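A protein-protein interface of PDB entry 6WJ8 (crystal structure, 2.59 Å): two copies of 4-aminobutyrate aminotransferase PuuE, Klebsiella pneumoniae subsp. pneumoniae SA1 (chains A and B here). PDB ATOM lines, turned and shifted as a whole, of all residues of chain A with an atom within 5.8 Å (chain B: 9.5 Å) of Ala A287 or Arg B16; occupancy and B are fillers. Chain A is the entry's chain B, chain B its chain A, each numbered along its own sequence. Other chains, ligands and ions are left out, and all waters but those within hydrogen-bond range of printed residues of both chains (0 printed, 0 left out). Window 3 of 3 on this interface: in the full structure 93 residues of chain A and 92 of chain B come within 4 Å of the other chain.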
ATOM      1  N   LYS A 103     -14.184 -26.092 -32.807  1.00  0.00           N
ATOM      2  CA  LYS A 103     -14.033 -24.675 -33.096  1.00  0.00           C
ATOM      3  C   LYS A 103     -13.342 -24.526 -34.441  1.00  0.00           C
ATOM      4  O   LYS A 103     -12.597 -25.411 -34.873  1.00  0.00           O
ATOM      5  CB  LYS A 103     -13.234 -23.949 -32.003  1.00  0.00           C
ATOM      6  CG  LYS A 103     -13.991 -23.764 -30.697  1.00  0.00           C
ATOM      7  CD  LYS A 103     -13.253 -22.825 -29.753  1.00  0.00           C
ATOM      8  CE  LYS A 103     -14.067 -22.556 -28.497  1.00  0.00           C
ATOM      9  NZ  LYS A 103     -13.415 -21.552 -27.613  1.00  0.00           N
ATOM     10  N   ILE A 120      -1.140 -24.424 -34.178  1.00  0.00           N
ATOM     11  CA  ILE A 120      -2.037 -24.875 -33.119  1.00  0.00           C
ATOM     12  C   ILE A 120      -1.497 -26.140 -32.466  1.00  0.00           C
ATOM     13  O   ILE A 120      -1.508 -26.278 -31.236  1.00  0.00           O
ATOM     14  CB  ILE A 120      -3.457 -25.087 -33.678  1.00  0.00           C
ATOM     15  CG1 ILE A 120      -4.144 -23.740 -33.918  1.00  0.00           C
ATOM     16  CG2 ILE A 120      -4.285 -25.951 -32.739  1.00  0.00           C
ATOM     17  CD1 ILE A 120      -5.294 -23.807 -34.898  1.00  0.00           C
ATOM     18  N   ALA A 123       1.399 -25.294 -30.178  1.00  0.00           N
ATOM     19  CA  ALA A 123       0.999 -24.572 -28.975  1.00  0.00           C
ATOM     20  C   ALA A 123       0.355 -25.503 -27.955  1.00  0.00           C
ATOM     21  O   ALA A 123       0.531 -25.324 -26.745  1.00  0.00           O
ATOM     22  CB  ALA A 123       0.047 -23.433 -29.340  1.00  0.00           C
ATOM     23  N   TYR A 124      -0.391 -26.505 -28.424  1.00  0.00           N
ATOM     24  CA  TYR A 124      -1.075 -27.412 -27.508  1.00  0.00           C
ATOM     25  C   TYR A 124      -0.101 -28.397 -26.876  1.00  0.00           C
ATOM     26  O   TYR A 124      -0.105 -28.596 -25.656  1.00  0.00           O
ATOM     27  CB  TYR A 124      -2.192 -28.152 -28.248  1.00  0.00           C
ATOM     28  CG  TYR A 124      -2.963 -29.135 -27.394  1.00  0.00           C
ATOM     29  CD1 TYR A 124      -3.989 -28.706 -26.562  1.00  0.00           C
ATOM     30  CD2 TYR A 124      -2.670 -30.492 -27.427  1.00  0.00           C
ATOM     31  CE1 TYR A 124      -4.698 -29.601 -25.781  1.00  0.00           C
ATOM     32  CE2 TYR A 124      -3.372 -31.394 -26.650  1.00  0.00           C
ATOM     33  CZ  TYR A 124      -4.384 -30.944 -25.830  1.00  0.00           C
ATOM     34  OH  TYR A 124      -5.086 -31.841 -25.057  1.00  0.00           O
ATOM     35  N   ALA A 282     -12.052 -28.399 -29.644  1.00  0.00           N
ATOM     36  CA  ALA A 282     -12.047 -27.057 -29.068  1.00  0.00           C
ATOM     37  C   ALA A 282     -10.880 -26.867 -28.106  1.00  0.00           C
ATOM     38  O   ALA A 282     -10.258 -25.798 -28.078  1.00  0.00           O
ATOM     39  CB  ALA A 282     -13.374 -26.786 -28.360  1.00  0.00           C
ATOM     40  N   GLU A 283     -10.568 -27.894 -27.314  1.00  0.00           N
ATOM     41  CA  GLU A 283      -9.454 -27.799 -26.377  1.00  0.00           C
ATOM     42  C   GLU A 283      -8.133 -27.583 -27.107  1.00  0.00           C
ATOM     43  O   GLU A 283      -7.279 -26.813 -26.651  1.00  0.00           O
ATOM     44  CB  GLU A 283      -9.397 -29.060 -25.515  1.00  0.00           C
ATOM     45  CG  GLU A 283      -8.216 -29.131 -24.564  1.00  0.00           C
ATOM     46  CD  GLU A 283      -8.096 -30.486 -23.897  1.00  0.00           C
ATOM     47  OE1 GLU A 283      -7.085 -30.724 -23.203  1.00  0.00           O
ATOM     48  OE2 GLU A 283      -9.015 -31.315 -24.068  1.00  0.00           O
ATOM     49  N   VAL A 284      -7.953 -28.245 -28.251  1.00  0.00           N
ATOM     50  CA  VAL A 284      -6.723 -28.081 -29.020  1.00  0.00           C
ATOM     51  C   VAL A 284      -6.693 -26.713 -29.690  1.00  0.00           C
ATOM     52  O   VAL A 284      -5.669 -26.021 -29.681  1.00  0.00           O
ATOM     53  CB  VAL A 284      -6.581 -29.216 -30.049  1.00  0.00           C
ATOM     54  CG1 VAL A 284      -5.292 -29.057 -30.841  1.00  0.00           C
ATOM     55  CG2 VAL A 284      -6.629 -30.572 -29.359  1.00  0.00           C
ATOM     56  N   MET A 285      -7.820 -26.302 -30.278  1.00  0.00           N
ATOM     57  CA  MET A 285      -7.865 -25.038 -31.005  1.00  0.00           C
ATOM     58  C   MET A 285      -7.602 -23.847 -30.092  1.00  0.00           C
ATOM     59  O   MET A 285      -7.043 -22.837 -30.536  1.00  0.00           O
ATOM     60  CB  MET A 285      -9.217 -24.880 -31.700  1.00  0.00           C
ATOM     61  CG  MET A 285      -9.484 -25.907 -32.788  1.00  0.00           C
ATOM     62  SD  MET A 285      -8.448 -25.667 -34.243  1.00  0.00           S
ATOM     63  CE  MET A 285      -9.236 -24.241 -34.983  1.00  0.00           C
ATOM     64  N   ASP A 286      -7.991 -23.943 -28.821  1.00  0.00           N
ATOM     65  CA  ASP A 286      -7.833 -22.843 -27.879  1.00  0.00           C
ATOM     66  C   ASP A 286      -6.424 -22.735 -27.310  1.00  0.00           C
ATOM     67  O   ASP A 286      -6.194 -21.895 -26.434  1.00  0.00           O
ATOM     68  CB  ASP A 286      -8.834 -22.990 -26.730  1.00  0.00           C
ATOM     69  CG  ASP A 286     -10.236 -22.577 -27.124  1.00  0.00           C
ATOM     70  OD1 ASP A 286     -10.374 -21.645 -27.944  1.00  0.00           O
ATOM     71  OD2 ASP A 286     -11.199 -23.184 -26.610  1.00  0.00           O
ATOM     72  N   ALA A 287      -5.480 -23.554 -27.781  1.00  0.00           N
ATOM     73  CA  ALA A 287      -4.136 -23.521 -27.205  1.00  0.00           C
ATOM     74  C   ALA A 287      -3.406 -22.214 -27.491  1.00  0.00           C
ATOM     75  O   ALA A 287      -2.833 -21.637 -26.551  1.00  0.00           O
ATOM     76  CB  ALA A 287      -3.338 -24.738 -27.679  1.00  0.00           C
ATOM     77  N   PRO A 288      -3.365 -21.696 -28.724  1.00  0.00           N
ATOM     78  CA  PRO A 288      -2.717 -20.395 -28.934  1.00  0.00           C
ATOM     79  C   PRO A 288      -3.465 -19.285 -28.208  1.00  0.00           C
ATOM     80  O   PRO A 288      -4.694 -19.290 -28.121  1.00  0.00           O
ATOM     81  CB  PRO A 288      -2.765 -20.211 -30.455  1.00  0.00           C
ATOM     82  CG  PRO A 288      -2.933 -21.582 -31.003  1.00  0.00           C
ATOM     83  CD  PRO A 288      -3.793 -22.289 -30.006  1.00  0.00           C
ATOM     84  N   ALA A 289      -2.703 -18.334 -27.681  1.00  0.00           N
ATOM     85  CA  ALA A 289      -3.256 -17.229 -26.917  1.00  0.00           C
ATOM     86  C   ALA A 289      -3.862 -16.181 -27.848  1.00  0.00           C
ATOM     87  O   ALA A 289      -3.600 -16.184 -29.054  1.00  0.00           O
ATOM     88  CB  ALA A 289      -2.166 -16.606 -26.049  1.00  0.00           C
ATOM     89  N   PRO A 290      -4.699 -15.288 -27.315  1.00  0.00           N
ATOM     90  CA  PRO A 290      -5.212 -14.182 -28.137  1.00  0.00           C
ATOM     91  C   PRO A 290      -4.076 -13.374 -28.748  1.00  0.00           C
ATOM     92  O   PRO A 290      -3.143 -12.957 -28.058  1.00  0.00           O
ATOM     93  CB  PRO A 290      -6.028 -13.354 -27.140  1.00  0.00           C
ATOM     94  CG  PRO A 290      -6.486 -14.347 -26.135  1.00  0.00           C
ATOM     95  CD  PRO A 290      -5.366 -15.347 -26.002  1.00  0.00           C
ATOM     96  N   GLY A 291      -4.163 -13.159 -30.059  1.00  0.00           N
ATOM     97  CA  GLY A 291      -3.132 -12.493 -30.816  1.00  0.00           C
ATOM     98  C   GLY A 291      -2.186 -13.427 -31.544  1.00  0.00           C
ATOM     99  O   GLY A 291      -1.515 -12.995 -32.488  1.00  0.00           O
ATOM    100  N   LEU A 293      -2.927 -16.015 -33.450  1.00  0.00           N
ATOM    101  CA  LEU A 293      -3.453 -16.430 -34.742  1.00  0.00           C
ATOM    102  C   LEU A 293      -4.027 -15.225 -35.475  1.00  0.00           C
ATOM    103  O   LEU A 293      -4.577 -14.309 -34.859  1.00  0.00           O
ATOM    104  CB  LEU A 293      -4.533 -17.505 -34.583  1.00  0.00           C
ATOM    105  CG  LEU A 293      -4.127 -18.732 -33.765  1.00  0.00           C
ATOM    106  CD1 LEU A 293      -5.323 -19.640 -33.524  1.00  0.00           C
ATOM    107  CD2 LEU A 293      -3.006 -19.487 -34.458  1.00  0.00           C
ATOM    108  N   ARG B  10     -19.459 -16.079 -31.193  1.00  0.00           N
ATOM    109  CA  ARG B  10     -18.100 -15.988 -31.717  1.00  0.00           C
ATOM    110  C   ARG B  10     -17.099 -16.649 -30.778  1.00  0.00           C
ATOM    111  O   ARG B  10     -16.135 -17.279 -31.229  1.00  0.00           O
ATOM    112  CB  ARG B  10     -17.733 -14.524 -31.948  1.00  0.00           C
ATOM    113  CG  ARG B  10     -16.319 -14.303 -32.442  1.00  0.00           C
ATOM    114  CD  ARG B  10     -15.911 -12.844 -32.315  1.00  0.00           C
ATOM    115  NE  ARG B  10     -15.874 -12.405 -30.924  1.00  0.00           N
ATOM    116  CZ  ARG B  10     -14.829 -12.564 -30.119  1.00  0.00           C
ATOM    117  NH1 ARG B  10     -13.730 -13.154 -30.566  1.00  0.00           N
ATOM    118  NH2 ARG B  10     -14.884 -12.135 -28.864  1.00  0.00           N
ATOM    119  N   GLN B  11     -17.313 -16.522 -29.468  1.00  0.00           N
ATOM    120  CA  GLN B  11     -16.377 -17.089 -28.504  1.00  0.00           C
ATOM    121  C   GLN B  11     -16.512 -18.602 -28.393  1.00  0.00           C
ATOM    122  O   GLN B  11     -15.524 -19.286 -28.101  1.00  0.00           O
ATOM    123  CB  GLN B  11     -16.579 -16.439 -27.134  1.00  0.00           C
ATOM    124  CG  GLN B  11     -16.059 -15.014 -27.048  1.00  0.00           C
ATOM    125  CD  GLN B  11     -16.601 -14.265 -25.847  1.00  0.00           C
ATOM    126  OE1 GLN B  11     -17.050 -14.870 -24.875  1.00  0.00           O
ATOM    127  NE2 GLN B  11     -16.561 -12.940 -25.909  1.00  0.00           N
ATOM    128  N   GLN B  12     -17.710 -19.142 -28.621  1.00  0.00           N
ATOM    129  CA  GLN B  12     -17.904 -20.583 -28.518  1.00  0.00           C
ATOM    130  C   GLN B  12     -17.531 -21.310 -29.803  1.00  0.00           C
ATOM    131  O   GLN B  12     -17.178 -22.494 -29.758  1.00  0.00           O
ATOM    132  CB  GLN B  12     -19.356 -20.898 -28.152  1.00  0.00           C
ATOM    133  CG  GLN B  12     -19.767 -20.443 -26.761  1.00  0.00           C
ATOM    134  CD  GLN B  12     -18.833 -20.948 -25.680  1.00  0.00           C
ATOM    135  OE1 GLN B  12     -18.296 -20.168 -24.895  1.00  0.00           O
ATOM    136  NE2 GLN B  12     -18.636 -22.261 -25.633  1.00  0.00           N
ATOM    137  N   ALA B  13     -17.592 -20.627 -30.947  1.00  0.00           N
ATOM    138  CA  ALA B  13     -17.407 -21.274 -32.239  1.00  0.00           C
ATOM    139  C   ALA B  13     -16.009 -21.107 -32.821  1.00  0.00           C
ATOM    140  O   ALA B  13     -15.596 -21.937 -33.637  1.00  0.00           O
ATOM    141  CB  ALA B  13     -18.432 -20.743 -33.248  1.00  0.00           C
ATOM    142  N   THR B  14     -15.280 -20.061 -32.442  1.00  0.00           N
ATOM    143  CA  THR B  14     -13.938 -19.846 -32.955  1.00  0.00           C
ATOM    144  C   THR B  14     -12.926 -19.896 -31.815  1.00  0.00           C
ATOM    145  O   THR B  14     -13.277 -19.625 -30.661  1.00  0.00           O
ATOM    146  CB  THR B  14     -13.828 -18.497 -33.682  1.00  0.00           C
ATOM    147  OG1 THR B  14     -13.576 -17.456 -32.731  1.00  0.00           O
ATOM    148  CG2 THR B  14     -15.108 -18.191 -34.444  1.00  0.00           C
ATOM    149  N   PRO B  15     -11.672 -20.249 -32.096  1.00  0.00           N
ATOM    150  CA  PRO B  15     -10.680 -20.331 -31.019  1.00  0.00           C
ATOM    151  C   PRO B  15     -10.329 -18.957 -30.474  1.00  0.00           C
ATOM    152  O   PRO B  15     -10.460 -17.938 -31.154  1.00  0.00           O
ATOM    153  CB  PRO B  15      -9.471 -20.981 -31.701  1.00  0.00           C
ATOM    154  CG  PRO B  15      -9.619 -20.616 -33.135  1.00  0.00           C
ATOM    155  CD  PRO B  15     -11.097 -20.629 -33.399  1.00  0.00           C
ATOM    156  N   ARG B  16      -9.877 -18.941 -29.219  1.00  0.00           N
ATOM    157  CA  ARG B  16      -9.442 -17.693 -28.604  1.00  0.00           C
ATOM    158  C   ARG B  16      -8.191 -17.130 -29.266  1.00  0.00           C
ATOM    159  O   ARG B  16      -7.872 -15.954 -29.058  1.00  0.00           O
ATOM    160  CB  ARG B  16      -9.184 -17.905 -27.111  1.00  0.00           C
ATOM    161  CG  ARG B  16      -7.746 -18.272 -26.789  1.00  0.00           C
ATOM    162  CD  ARG B  16      -7.641 -19.110 -25.530  1.00  0.00           C
ATOM    163  NE  ARG B  16      -6.300 -19.661 -25.368  1.00  0.00           N
ATOM    164  CZ  ARG B  16      -5.436 -19.262 -24.441  1.00  0.00           C
ATOM    165  NH1 ARG B  16      -5.773 -18.305 -23.588  1.00  0.00           N
ATOM    166  NH2 ARG B  16      -4.235 -19.820 -24.368  1.00  0.00           N
ATOM    167  N   GLY B  17      -7.483 -17.938 -30.059  1.00  0.00           N
ATOM    168  CA  GLY B  17      -6.249 -17.476 -30.669  1.00  0.00           C
ATOM    169  C   GLY B  17      -6.446 -16.339 -31.652  1.00  0.00           C
ATOM    170  O   GLY B  17      -5.536 -15.533 -31.862  1.00  0.00           O
ATOM    171  N   VAL B  18      -7.623 -16.256 -32.269  1.00  0.00           N
ATOM    172  CA  VAL B  18      -7.937 -15.157 -33.185  1.00  0.00           C
ATOM    173  C   VAL B  18      -8.544 -14.045 -32.333  1.00  0.00           C
ATOM    174  O   VAL B  18      -9.753 -13.982 -32.106  1.00  0.00           O
ATOM    175  CB  VAL B  18      -8.849 -15.597 -34.330  1.00  0.00           C
ATOM    176  CG1 VAL B  18      -8.043 -16.342 -35.383  1.00  0.00           C
ATOM    177  CG2 VAL B  18      -9.984 -16.477 -33.831  1.00  0.00           C
ATOM    178  N   GLY B  19      -7.680 -13.160 -31.843  1.00  0.00           N
ATOM    179  CA  GLY B  19      -8.147 -12.040 -31.052  1.00  0.00           C
ATOM    180  C   GLY B  19      -8.973 -11.072 -31.876  1.00  0.00           C
ATOM    181  O   GLY B  19      -8.811 -10.949 -33.090  1.00  0.00           O
ATOM    182  N   VAL B  20      -9.879 -10.376 -31.197  1.00  0.00           N
ATOM    183  CA  VAL B  20     -10.792  -9.431 -31.829  1.00  0.00           C
ATOM    184  C   VAL B  20     -10.766  -8.142 -31.018  1.00  0.00           C
ATOM    185  O   VAL B  20     -11.036  -8.159 -29.812  1.00  0.00           O
ATOM    186  CB  VAL B  20     -12.222  -9.989 -31.925  1.00  0.00           C
ATOM    187  CG1 VAL B  20     -13.177  -8.908 -32.369  1.00  0.00           C
ATOM    188  CG2 VAL B  20     -12.266 -11.172 -32.885  1.00  0.00           C
ATOM    189  N   PRO B 153       2.660 -10.953 -29.513  1.00  0.00           N
ATOM    190  CA  PRO B 153       2.176 -12.320 -29.311  1.00  0.00           C
ATOM    191  C   PRO B 153       2.374 -13.195 -30.545  1.00  0.00           C
ATOM    192  O   PRO B 153       1.791 -14.277 -30.634  1.00  0.00           O
ATOM    193  CB  PRO B 153       0.692 -12.102 -29.045  1.00  0.00           C
ATOM    194  CG  PRO B 153       0.350 -10.952 -29.969  1.00  0.00           C
ATOM    195  CD  PRO B 153       1.614 -10.105 -30.114  1.00  0.00           C
ATOM    196  N   ILE B 156       4.649 -16.535 -29.755  1.00  0.00           N
ATOM    197  CA  ILE B 156       4.606 -17.188 -28.450  1.00  0.00           C
ATOM    198  C   ILE B 156       3.961 -18.561 -28.624  1.00  0.00           C
ATOM    199  O   ILE B 156       2.759 -18.666 -28.879  1.00  0.00           O
ATOM    200  CB  ILE B 156       3.852 -16.345 -27.417  1.00  0.00           C
ATOM    201  CG1 ILE B 156       4.505 -14.968 -27.270  1.00  0.00           C
ATOM    202  CG2 ILE B 156       3.806 -17.066 -26.077  1.00  0.00           C
ATOM    203  CD1 ILE B 156       5.690 -14.946 -26.328  1.00  0.00           C
ATOM    204  N   GLY B 157       4.765 -19.617 -28.497  1.00  0.00           N
ATOM    205  CA  GLY B 157       4.267 -20.976 -28.526  1.00  0.00           C
ATOM    206  C   GLY B 157       4.375 -21.690 -29.856  1.00  0.00           C
ATOM    207  O   GLY B 157       3.877 -22.817 -29.972  1.00  0.00           O
ATOM    208  N   PHE B 158       5.011 -21.085 -30.857  1.00  0.00           N
ATOM    209  CA  PHE B 158       5.096 -21.673 -32.187  1.00  0.00           C
ATOM    210  C   PHE B 158       6.507 -22.098 -32.567  1.00  0.00           C
ATOM    211  O   PHE B 158       6.711 -22.583 -33.685  1.00  0.00           O
ATOM    212  CB  PHE B 158       4.545 -20.692 -33.227  1.00  0.00           C
ATOM    213  CG  PHE B 158       3.209 -20.116 -32.859  1.00  0.00           C
ATOM    214  CD1 PHE B 158       2.153 -20.948 -32.521  1.00  0.00           C
ATOM    215  CD2 PHE B 158       3.010 -18.747 -32.838  1.00  0.00           C
ATOM    216  CE1 PHE B 158       0.923 -20.424 -32.175  1.00  0.00           C
ATOM    217  CE2 PHE B 158       1.781 -18.216 -32.493  1.00  0.00           C
ATOM    218  CZ  PHE B 158       0.736 -19.057 -32.162  1.00  0.00           C
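Among the printed residues, merely in contact across the chains: Lys A103 with Gln B12 (3.4 Å), Lys A103 with Ala B13 (3.2 Å), Lys A103 with Thr B14 (3.3 Å), Lys A103 with Pro B15 (3.8 Å), Ala A123 with Gly B157 (3.5 Å), Met A285 with Pro B15 (3.3 Å), Asp A286 with Pro B15 (3.4 Å), Pro A288 with Gly B17 (3.5 Å), Ala A289 with Arg B16 (3.8 Å), Pro A290 with Arg B16 (3.3 Å), Pro A290 with Gly B17 (3.98 Å), Gly A291 with Gly B19 (3.9 Å), Gly A291 with Pro B153 (3.7 Å) and Leu A293 with Val B18 (3.8 Å).
Of the printed residues of chain B, Ala A123 touches Gly B157 (3.5 Å). Of chain B, only Pro B15 and Arg B16 come within 4 Å of Asp A286. Printed residues of chain B within 4 Å of Ala A287: Arg B16 (3.2 Å). Pro A288 touches just these residues of chain B: Arg B16 and Gly B17. Of chain B, only Arg B16 and Gly B17 come within 4 Å of Ala A289. Of the printed residues of chain B, Pro A290 touches Arg B16 and Gly B17. Arg B16 touches just these residues of chain A: Asp A286, Ala A287, Pro A288, Ala A289 and Pro A290. Printed residues of chain A within 4 Å of Gly B17: Pro A288 (3.5 Å), Ala A289 (3.4 Å), Pro A290 (3.98 Å), Gly A291 (3.3 Å) and Leu A293 (3.1 Å). The nearest residue of chain A that does not touch Arg B16 is Lys A103 (4.7 Å).
NE of Arg B16 sits at hydrogen-bond distance from O of Asp A286, 2.5 Å away. The guanidinium group (NH2) of Arg B16 lies within hydrogen-bond range of the backbone carbonyl oxygen (O) of Ala A287, at 3.2 Å. N of Gly A291 is in hydrogen-bond range of O of Gly B17, at 3.3 Å. O of Gly B17 sits close to O of Ala A289 (3.5 Å). O of Pro A288 lies within hydrogen-bond range of NE of Arg B16 (3.2 Å). The backbone carbonyl oxygen of Gln B11 sits at hydrogen-bond distance from the side-chain amino group of Lys A103, 3.1 Å away. N of Leu A293 sits at hydrogen-bond distance from O of Gly B17.
Hydrophobic or aromatic side chains of chain B that line the printed part of chain A: Pro B15, Val B18 and Pro B153. Along chain B the printed residues that touch a printed residue of chain A span positions 11 to 157. Of the 15 printed residues of chain A, 10 touch a printed residue of chain B.
No position is printed for both chains. Of the 21 pairs that touch across the chains among the printed residues, none has its exchanged pair printed and touching as well.
The guanidinium group (NH2) of Arg B10 sits close to the side-chain amide nitrogen (NE2) of Gln B11, 3.5 Å away. O of Arg B10 sits at hydrogen-bond distance from OG1 of Thr B14, at 3.0 Å. OD2 of Asp A286 is in salt-bridge range of NZ of Lys A103.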
